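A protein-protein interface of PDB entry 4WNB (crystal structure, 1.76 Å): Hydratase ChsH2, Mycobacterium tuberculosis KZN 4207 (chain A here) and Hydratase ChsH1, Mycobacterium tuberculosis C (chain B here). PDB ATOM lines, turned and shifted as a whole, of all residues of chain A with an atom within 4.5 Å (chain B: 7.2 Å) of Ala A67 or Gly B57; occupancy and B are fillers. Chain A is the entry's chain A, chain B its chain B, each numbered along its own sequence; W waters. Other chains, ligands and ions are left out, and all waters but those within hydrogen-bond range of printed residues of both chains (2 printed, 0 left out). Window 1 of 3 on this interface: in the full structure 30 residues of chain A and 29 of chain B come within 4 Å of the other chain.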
ATOM      1  N   TRP A  37      29.907  13.091  -2.552  1.00  0.00           N
ATOM      2  CA  TRP A  37      28.955  12.943  -3.651  1.00  0.00           C
ATOM      3  C   TRP A  37      28.087  11.690  -3.472  1.00  0.00           C
ATOM      4  O   TRP A  37      26.864  11.784  -3.548  1.00  0.00           O
ATOM      5  CB  TRP A  37      29.722  12.920  -4.991  1.00  0.00           C
ATOM      6  CG  TRP A  37      28.924  12.966  -6.254  1.00  0.00           C
ATOM      7  CD1 TRP A  37      28.657  14.074  -7.025  1.00  0.00           C
ATOM      8  CD2 TRP A  37      28.363  11.848  -6.953  1.00  0.00           C
ATOM      9  NE1 TRP A  37      27.947  13.709  -8.157  1.00  0.00           N
ATOM     10  CE2 TRP A  37      27.738  12.354  -8.126  1.00  0.00           C
ATOM     11  CE3 TRP A  37      28.300  10.471  -6.690  1.00  0.00           C
ATOM     12  CZ2 TRP A  37      27.065  11.526  -9.031  1.00  0.00           C
ATOM     13  CZ3 TRP A  37      27.627   9.652  -7.587  1.00  0.00           C
ATOM     14  CH2 TRP A  37      27.025  10.183  -8.745  1.00  0.00           C
ATOM     15  N   ILE A  41      24.069  11.843  -3.066  1.00  0.00           N
ATOM     16  CA  ILE A  41      23.306  11.224  -4.158  1.00  0.00           C
ATOM     17  C   ILE A  41      22.607   9.956  -3.643  1.00  0.00           C
ATOM     18  O   ILE A  41      21.551   9.551  -4.139  1.00  0.00           O
ATOM     19  CB  ILE A  41      24.214  10.877  -5.367  1.00  0.00           C
ATOM     20  CG1 ILE A  41      24.835  12.143  -5.970  1.00  0.00           C
ATOM     21  CG2 ILE A  41      23.441  10.108  -6.448  1.00  0.00           C
ATOM     22  CD1 ILE A  41      23.811  13.164  -6.503  1.00  0.00           C
ATOM     23  N   PRO A  65      32.719   7.846  -9.788  1.00  0.00           N
ATOM     24  CA  PRO A  65      31.471   7.803 -10.551  1.00  0.00           C
ATOM     25  C   PRO A  65      31.637   8.557 -11.865  1.00  0.00           C
ATOM     26  O   PRO A  65      32.112   9.691 -11.862  1.00  0.00           O
ATOM     27  CB  PRO A  65      30.461   8.505  -9.631  1.00  0.00           C
ATOM     28  CG  PRO A  65      31.022   8.318  -8.251  1.00  0.00           C
ATOM     29  CD  PRO A  65      32.516   8.407  -8.434  1.00  0.00           C
ATOM     30  N   PRO A  66      31.304   7.911 -12.980  1.00  0.00           N
ATOM     31  CA  PRO A  66      31.405   8.595 -14.273  1.00  0.00           C
ATOM     32  C   PRO A  66      30.688   9.947 -14.262  1.00  0.00           C
ATOM     33  O   PRO A  66      31.225  10.920 -14.788  1.00  0.00           O
ATOM     34  CB  PRO A  66      30.734   7.620 -15.231  1.00  0.00           C
ATOM     35  CG  PRO A  66      31.026   6.269 -14.625  1.00  0.00           C
ATOM     36  CD  PRO A  66      31.027   6.468 -13.121  1.00  0.00           C
ATOM     37  N   ALA A  67      29.516  10.002 -13.637  1.00  0.00           N
ATOM     38  CA  ALA A  67      28.706  11.218 -13.595  1.00  0.00           C
ATOM     39  C   ALA A  67      29.327  12.316 -12.727  1.00  0.00           C
ATOM     40  O   ALA A  67      28.751  13.395 -12.609  1.00  0.00           O
ATOM     41  CB  ALA A  67      27.291  10.894 -13.090  1.00  0.00           C
ATOM     42  N   MET A  68      30.494  12.053 -12.132  1.00  0.00           N
ATOM     43  CA  MET A  68      31.208  13.097 -11.395  1.00  0.00           C
ATOM     44  C   MET A  68      32.143  13.914 -12.301  1.00  0.00           C
ATOM     45  O   MET A  68      32.770  14.857 -11.832  1.00  0.00           O
ATOM     46  CB  MET A  68      32.017  12.497 -10.232  1.00  0.00           C
ATOM     47  CG  MET A  68      31.198  12.284  -8.972  1.00  0.00           C
ATOM     48  SD  MET A  68      32.253  12.008  -7.511  1.00  0.00           S
ATOM     49  CE  MET A  68      32.704  13.699  -7.131  1.00  0.00           C
ATOM     50  N   ILE A  69      32.221  13.577 -13.587  1.00  0.00           N
ATOM     51  CA  ILE A  69      33.290  14.147 -14.418  1.00  0.00           C
ATOM     52  C   ILE A  69      33.211  15.692 -14.404  1.00  0.00           C
ATOM     53  O   ILE A  69      34.215  16.378 -14.233  1.00  0.00           O
ATOM     54  CB  ILE A  69      33.265  13.575 -15.898  1.00  0.00           C
ATOM     55  CG1 ILE A  69      34.417  14.164 -16.711  1.00  0.00           C
ATOM     56  CG2 ILE A  69      31.941  13.839 -16.603  1.00  0.00           C
ATOM     57  CD1 ILE A  69      35.785  13.673 -16.253  1.00  0.00           C
ATOM     58  N   GLN A 109      26.383  13.184 -21.856  1.00  0.00           N
ATOM     59  CA  GLN A 109      27.775  12.931 -21.484  1.00  0.00           C
ATOM     60  C   GLN A 109      28.252  11.571 -21.960  1.00  0.00           C
ATOM     61  O   GLN A 109      27.521  10.602 -21.860  1.00  0.00           O
ATOM     62  CB  GLN A 109      27.965  13.017 -19.966  1.00  0.00           C
ATOM     63  CG  GLN A 109      27.580  14.358 -19.403  1.00  0.00           C
ATOM     64  CD  GLN A 109      27.994  14.549 -17.961  1.00  0.00           C
ATOM     65  OE1 GLN A 109      28.128  13.587 -17.188  1.00  0.00           O
ATOM     66  NE2 GLN A 109      28.218  15.802 -17.589  1.00  0.00           N
ATOM     67  N   TYR A 111      31.444   8.795 -21.547  1.00  0.00           N
ATOM     68  CA  TYR A 111      32.560   8.393 -20.696  1.00  0.00           C
ATOM     69  C   TYR A 111      33.402   7.334 -21.390  1.00  0.00           C
ATOM     70  O   TYR A 111      32.961   6.192 -21.549  1.00  0.00           O
ATOM     71  CB  TYR A 111      32.046   7.854 -19.355  1.00  0.00           C
ATOM     72  CG  TYR A 111      30.922   8.684 -18.785  1.00  0.00           C
ATOM     73  CD1 TYR A 111      31.152   9.974 -18.315  1.00  0.00           C
ATOM     74  CD2 TYR A 111      29.629   8.188 -18.728  1.00  0.00           C
ATOM     75  CE1 TYR A 111      30.127  10.740 -17.797  1.00  0.00           C
ATOM     76  CE2 TYR A 111      28.596   8.949 -18.207  1.00  0.00           C
ATOM     77  CZ  TYR A 111      28.852  10.226 -17.748  1.00  0.00           C
ATOM     78  OH  TYR A 111      27.825  10.979 -17.227  1.00  0.00           O
ATOM     79  N   THR B  27      27.937  18.401  -5.880  1.00  0.00           N
ATOM     80  CA  THR B  27      28.323  18.471  -7.303  1.00  0.00           C
ATOM     81  C   THR B  27      29.052  19.794  -7.600  1.00  0.00           C
ATOM     82  O   THR B  27      29.337  20.108  -8.762  1.00  0.00           O
ATOM     83  CB  THR B  27      27.125  18.327  -8.256  1.00  0.00           C
ATOM     84  OG1 THR B  27      26.205  19.416  -8.077  1.00  0.00           O
ATOM     85  CG2 THR B  27      26.411  16.999  -8.017  1.00  0.00           C
ATOM     86  N   ASN B  51      19.519  20.309  -9.208  1.00  0.00           N
ATOM     87  CA  ASN B  51      20.361  20.740 -10.322  1.00  0.00           C
ATOM     88  C   ASN B  51      20.594  19.613 -11.336  1.00  0.00           C
ATOM     89  O   ASN B  51      20.238  18.461 -11.106  1.00  0.00           O
ATOM     90  CB  ASN B  51      21.698  21.326  -9.803  1.00  0.00           C
ATOM     91  CG  ASN B  51      22.730  20.269  -9.417  1.00  0.00           C
ATOM     92  OD1 ASN B  51      22.392  19.168  -9.023  1.00  0.00           O
ATOM     93  ND2 ASN B  51      24.016  20.630  -9.520  1.00  0.00           N
ATOM     94  N   ILE B  52      21.170  19.958 -12.474  1.00  0.00           N
ATOM     95  CA  ILE B  52      21.273  19.020 -13.573  1.00  0.00           C
ATOM     96  C   ILE B  52      22.316  17.923 -13.269  1.00  0.00           C
ATOM     97  O   ILE B  52      22.130  16.762 -13.657  1.00  0.00           O
ATOM     98  CB  ILE B  52      21.600  19.780 -14.884  1.00  0.00           C
ATOM     99  CG1 ILE B  52      20.420  20.697 -15.256  1.00  0.00           C
ATOM    100  CG2 ILE B  52      21.929  18.814 -16.034  1.00  0.00           C
ATOM    101  CD1 ILE B  52      20.776  21.841 -16.251  1.00  0.00           C
ATOM    102  N   LEU B  53      23.385  18.275 -12.549  1.00  0.00           N
ATOM    103  CA  LEU B  53      24.420  17.285 -12.224  1.00  0.00           C
ATOM    104  C   LEU B  53      23.885  16.219 -11.280  1.00  0.00           C
ATOM    105  O   LEU B  53      24.323  15.074 -11.325  1.00  0.00           O
ATOM    106  CB  LEU B  53      25.657  17.949 -11.626  1.00  0.00           C
ATOM    107  CG  LEU B  53      26.727  18.317 -12.657  1.00  0.00           C
ATOM    108  CD1 LEU B  53      27.942  19.019 -12.041  1.00  0.00           C
ATOM    109  CD2 LEU B  53      27.149  17.064 -13.439  1.00  0.00           C
ATOM    110  N   THR B  54      22.938  16.592 -10.432  1.00  0.00           N
ATOM    111  CA  THR B  54      22.302  15.614  -9.562  1.00  0.00           C
ATOM    112  C   THR B  54      21.387  14.713 -10.399  1.00  0.00           C
ATOM    113  O   THR B  54      21.330  13.494 -10.175  1.00  0.00           O
ATOM    114  CB  THR B  54      21.516  16.309  -8.435  1.00  0.00           C
ATOM    115  OG1 THR B  54      22.429  17.056  -7.616  1.00  0.00           O
ATOM    116  CG2 THR B  54      20.744  15.318  -7.574  1.00  0.00           C
ATOM    117  N   ASP B  55      20.677  15.294 -11.364  1.00  0.00           N
ATOM    118  CA  ASP B  55      19.899  14.470 -12.304  1.00  0.00           C
ATOM    119  C   ASP B  55      20.771  13.390 -12.931  1.00  0.00           C
ATOM    120  O   ASP B  55      20.392  12.221 -12.986  1.00  0.00           O
ATOM    121  CB  ASP B  55      19.275  15.302 -13.446  1.00  0.00           C
ATOM    122  CG  ASP B  55      18.027  16.079 -13.027  1.00  0.00           C
ATOM    123  OD1 ASP B  55      17.351  15.686 -12.053  1.00  0.00           O
ATOM    124  OD2 ASP B  55      17.713  17.085 -13.706  1.00  0.00           O
ATOM    125  N   THR B  56      21.935  13.794 -13.432  1.00  0.00           N
ATOM    126  CA  THR B  56      22.843  12.865 -14.084  1.00  0.00           C
ATOM    127  C   THR B  56      23.267  11.765 -13.103  1.00  0.00           C
ATOM    128  O   THR B  56      23.300  10.578 -13.439  1.00  0.00           O
ATOM    129  CB  THR B  56      24.080  13.604 -14.616  1.00  0.00           C
ATOM    130  OG1 THR B  56      23.661  14.700 -15.437  1.00  0.00           O
ATOM    131  CG2 THR B  56      24.950  12.685 -15.439  1.00  0.00           C
ATOM    132  N   GLY B  57      23.569  12.172 -11.879  1.00  0.00           N
ATOM    133  CA  GLY B  57      24.043  11.233 -10.878  1.00  0.00           C
ATOM    134  C   GLY B  57      22.977  10.239 -10.449  1.00  0.00           C
ATOM    135  O   GLY B  57      23.277   9.072 -10.184  1.00  0.00           O
ATOM    136  N   LEU B  58      21.733  10.701 -10.363  1.00  0.00           N
ATOM    137  CA  LEU B  58      20.633   9.815  -9.978  1.00  0.00           C
ATOM    138  C   LEU B  58      20.281   8.835 -11.083  1.00  0.00           C
ATOM    139  O   LEU B  58      19.942   7.681 -10.816  1.00  0.00           O
ATOM    140  CB  LEU B  58      19.401  10.625  -9.606  1.00  0.00           C
ATOM    141  CG  LEU B  58      19.532  11.495  -8.357  1.00  0.00           C
ATOM    142  CD1 LEU B  58      18.286  12.338  -8.212  1.00  0.00           C
ATOM    143  CD2 LEU B  58      19.749  10.606  -7.127  1.00  0.00           C
ATOM    144  N   VAL B  59      20.360   9.296 -12.328  1.00  0.00           N
ATOM    145  CA  VAL B  59      20.087   8.423 -13.450  1.00  0.00           C
ATOM    146  C   VAL B  59      21.121   7.314 -13.452  1.00  0.00           C
ATOM    147  O   VAL B  59      20.782   6.131 -13.583  1.00  0.00           O
ATOM    148  CB  VAL B  59      20.104   9.190 -14.784  1.00  0.00           C
ATOM    149  CG1 VAL B  59      20.120   8.218 -15.954  1.00  0.00           C
ATOM    150  CG2 VAL B  59      18.894  10.093 -14.866  1.00  0.00           C
ATOM    151  N   GLN B  60      22.378   7.697 -13.270  1.00  0.00           N
ATOM    152  CA  GLN B  60      23.467   6.732 -13.136  1.00  0.00           C
ATOM    153  C   GLN B  60      23.231   5.724 -12.002  1.00  0.00           C
ATOM    154  O   GLN B  60      23.372   4.501 -12.187  1.00  0.00           O
ATOM    155  CB  GLN B  60      24.777   7.462 -12.895  1.00  0.00           C
ATOM    156  CG  GLN B  60      25.953   6.537 -12.680  1.00  0.00           C
ATOM    157  CD  GLN B  60      27.216   7.289 -12.346  1.00  0.00           C
ATOM    158  OE1 GLN B  60      27.926   7.761 -13.229  1.00  0.00           O
ATOM    159  NE2 GLN B  60      27.502   7.407 -11.068  1.00  0.00           N
ATOM    160  N   ARG B  61      22.875   6.246 -10.830  1.00  0.00           N
ATOM    161  CA  ARG B  61      22.562   5.408  -9.672  1.00  0.00           C
ATOM    162  C   ARG B  61      21.407   4.438  -9.934  1.00  0.00           C
ATOM    163  O   ARG B  61      21.485   3.250  -9.594  1.00  0.00           O
ATOM    164  CB  ARG B  61      22.224   6.279  -8.465  1.00  0.00           C
ATOM    165  CG  ARG B  61      21.809   5.458  -7.234  1.00  0.00           C
ATOM    166  CD  ARG B  61      21.221   6.356  -6.152  1.00  0.00           C
ATOM    167  NE  ARG B  61      20.269   5.623  -5.313  1.00  0.00           N
ATOM    168  CZ  ARG B  61      19.477   6.195  -4.413  1.00  0.00           C
ATOM    169  NH1 ARG B  61      19.519   7.508  -4.225  1.00  0.00           N
ATOM    170  NH2 ARG B  61      18.646   5.451  -3.691  1.00  0.00           N
ATOM    171  N   TYR B  62      20.342   4.955 -10.536  1.00  0.00           N
ATOM    172  CA  TYR B  62      19.145   4.174 -10.833  1.00  0.00           C
ATOM    173  C   TYR B  62      19.444   2.966 -11.716  1.00  0.00           C
ATOM    174  O   TYR B  62      18.926   1.870 -11.484  1.00  0.00           O
ATOM    175  CB  TYR B  62      18.090   5.060 -11.501  1.00  0.00           C
ATOM    176  CG  TYR B  62      16.800   4.342 -11.824  1.00  0.00           C
ATOM    177  CD1 TYR B  62      15.969   3.878 -10.810  1.00  0.00           C
ATOM    178  CD2 TYR B  62      16.406   4.134 -13.144  1.00  0.00           C
ATOM    179  CE1 TYR B  62      14.783   3.219 -11.096  1.00  0.00           C
ATOM    180  CE2 TYR B  62      15.218   3.481 -13.442  1.00  0.00           C
ATOM    181  CZ  TYR B  62      14.412   3.023 -12.411  1.00  0.00           C
ATOM    182  OH  TYR B  62      13.230   2.370 -12.698  1.00  0.00           O
ATOM    183  N   VAL B  63      20.295   3.164 -12.716  1.00  0.00           N
ATOM    184  CA  VAL B  63      20.635   2.091 -13.645  1.00  0.00           C
ATOM    185  C   VAL B  63      21.634   1.114 -13.026  1.00  0.00           C
ATOM    186  O   VAL B  63      21.512  -0.096 -13.213  1.00  0.00           O
ATOM    187  CB  VAL B  63      21.184   2.669 -14.975  1.00  0.00           C
ATOM    188  CG1 VAL B  63      21.636   1.565 -15.906  1.00  0.00           C
ATOM    189  CG2 VAL B  63      20.119   3.501 -15.639  1.00  0.00           C
ATOM    190  N   THR B  64      22.599   1.609 -12.255  1.00  0.00           N
ATOM    191  CA  THR B  64      23.541   0.689 -11.621  1.00  0.00           C
ATOM    192  C   THR B  64      22.919  -0.014 -10.410  1.00  0.00           C
ATOM    193  O   THR B  64      23.349  -1.110 -10.045  1.00  0.00           O
ATOM    194  CB  THR B  64      24.838   1.386 -11.192  1.00  0.00           C
ATOM    195  OG1 THR B  64      24.546   2.393 -10.218  1.00  0.00           O
ATOM    196  CG2 THR B  64      25.516   2.021 -12.393  1.00  0.00           C
ATOM    197  N   ILE B  73      29.229   2.216 -17.267  1.00  0.00           N
ATOM    198  CA  ILE B  73      28.405   3.257 -17.847  1.00  0.00           C
ATOM    199  C   ILE B  73      29.141   3.935 -18.997  1.00  0.00           C
ATOM    200  O   ILE B  73      30.220   4.499 -18.792  1.00  0.00           O
ATOM    201  CB  ILE B  73      28.025   4.324 -16.793  1.00  0.00           C
ATOM    202  CG1 ILE B  73      27.251   3.685 -15.633  1.00  0.00           C
ATOM    203  CG2 ILE B  73      27.245   5.471 -17.450  1.00  0.00           C
ATOM    204  CD1 ILE B  73      25.983   2.980 -16.055  1.00  0.00           C
ATOM    205  N   ILE B  76      25.372   8.908 -20.714  1.00  0.00           N
ATOM    206  CA  ILE B  76      24.106   9.338 -20.129  1.00  0.00           C
ATOM    207  C   ILE B  76      23.599  10.577 -20.860  1.00  0.00           C
ATOM    208  O   ILE B  76      24.249  11.625 -20.853  1.00  0.00           O
ATOM    209  CB  ILE B  76      24.236   9.648 -18.625  1.00  0.00           C
ATOM    210  CG1 ILE B  76      24.675   8.391 -17.853  1.00  0.00           C
ATOM    211  CG2 ILE B  76      22.925  10.206 -18.075  1.00  0.00           C
ATOM    212  CD1 ILE B  76      24.867   8.635 -16.343  1.00  0.00           C
ATOM    213  N   LEU B  78      20.499  13.299 -21.298  1.00  0.00           N
ATOM    214  CA  LEU B  78      19.353  13.873 -20.608  1.00  0.00           C
ATOM    215  C   LEU B  78      18.590  14.829 -21.500  1.00  0.00           C
ATOM    216  O   LEU B  78      19.190  15.696 -22.143  1.00  0.00           O
ATOM    217  CB  LEU B  78      19.786  14.624 -19.351  1.00  0.00           C
ATOM    218  CG  LEU B  78      20.560  13.893 -18.258  1.00  0.00           C
ATOM    219  CD1 LEU B  78      20.684  14.825 -17.070  1.00  0.00           C
ATOM    220  CD2 LEU B  78      19.868  12.583 -17.875  1.00  0.00           C
HETATM  221  O   HOH W   1      32.543   4.199 -19.495  1.00  0.00           O
HETATM  222  O   HOH W   2      26.994  14.605 -10.754  1.00  0.00           O
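The side-chain amide oxygen (OE1) of Gln B60 sits at hydrogen-bond distance from the backbone NH (N) of Ala A67, at 2.8 Å. The guanidinium group of Arg B61 is in hydrogen-bond range of the backbone carbonyl oxygen of Ile A41 (2.9 Å). The backbone NH of Gln A109 is in hydrogen-bond range of the backbone carbonyl oxygen of Ile B76 (2.8 Å). The side-chain amide oxygen (OE1) of Gln B60 lies close to the backbone nitrogen (N) of Pro A66 (3.4 Å).
OG1 of Thr B54 sits at hydrogen-bond distance from OD1 of Asn B51, at 2.5 Å. O of Arg B61 lies within hydrogen-bond range of OG1 of Thr B64. The side-chain amide oxygen of Gln A109 is in hydrogen-bond range of the side-chain hydroxyl of Tyr A111, 2.6 Å away. The side-chain hydroxyl (OG1) of Thr B56 sits at hydrogen-bond distance from the backbone carbonyl oxygen (O) of Ile B52 (3.1 Å). ND2 of Asn B51 lies within hydrogen-bond range of OG1 of Thr B27, at 2.9 Å. OG1 of Thr B64 lies within hydrogen-bond range of O of Gln B60 (3.1 Å).
Thr B27 touches Trp A37. Trp A37 touches Gln B60 (CH2 to NE2, 3.7 Å). Ile A41 touches Gly B57. Ile A41 touches Leu B58 (O to CD2, 3.6 Å). Gln B60 touches Pro A65 (NE2 to CB, 3.5 Å). Ala A67 touches Thr B56. Gly B57 touches Ala A67. Gln A109 touches Thr B56. Thr B56 touches Tyr A111 (CG2 to OH, 3.8 Å). CD2 of Tyr A111 touches O of Ile B73, 3.7 Å away.
Printed residues of chain B within 4 Å of Ala A67: Thr B56 (3.8 Å), Gly B57 (3.9 Å) and Gln B60 (2.8 Å). Of chain A, only Trp A37, Ile A41 and Ala A67 come within 4 Å of Gly B57. Printed residues of chain B within 4 Å of Tyr A111: Thr B56 (3.8 Å), Ile B73 (3.7 Å) and Ile B76 (3.9 Å). Of the printed residues of chain A, Ile B76 touches Gln A109 (2.8 Å) and Tyr A111 (3.9 Å). Of the printed residues of chain B, Pro A65 touches Gln B60 (3.5 Å). Printed residues of chain A within 4 Å of Leu B58: Ile A41. Asp B55 touches none of the printed residues of chain A. The nearest printed residue of chain B that does not touch Ala A67 is Leu B53 (4.1 Å).
Printed residues of chain B that touch a printed residue of chain A: Thr B27, Thr B54, Thr B56, Gly B57, Leu B58, Gln B60, Arg B61, Ile B73 and Ile B76.
Water W1 lies within hydrogen-bond range of the backbone carbonyl oxygen of Ile B73 and the backbone carbonyl oxygen of Tyr A111. Water W2 lies within hydrogen-bond range of O of Leu B53, O of Ala A67 and NE1 of Trp A37.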
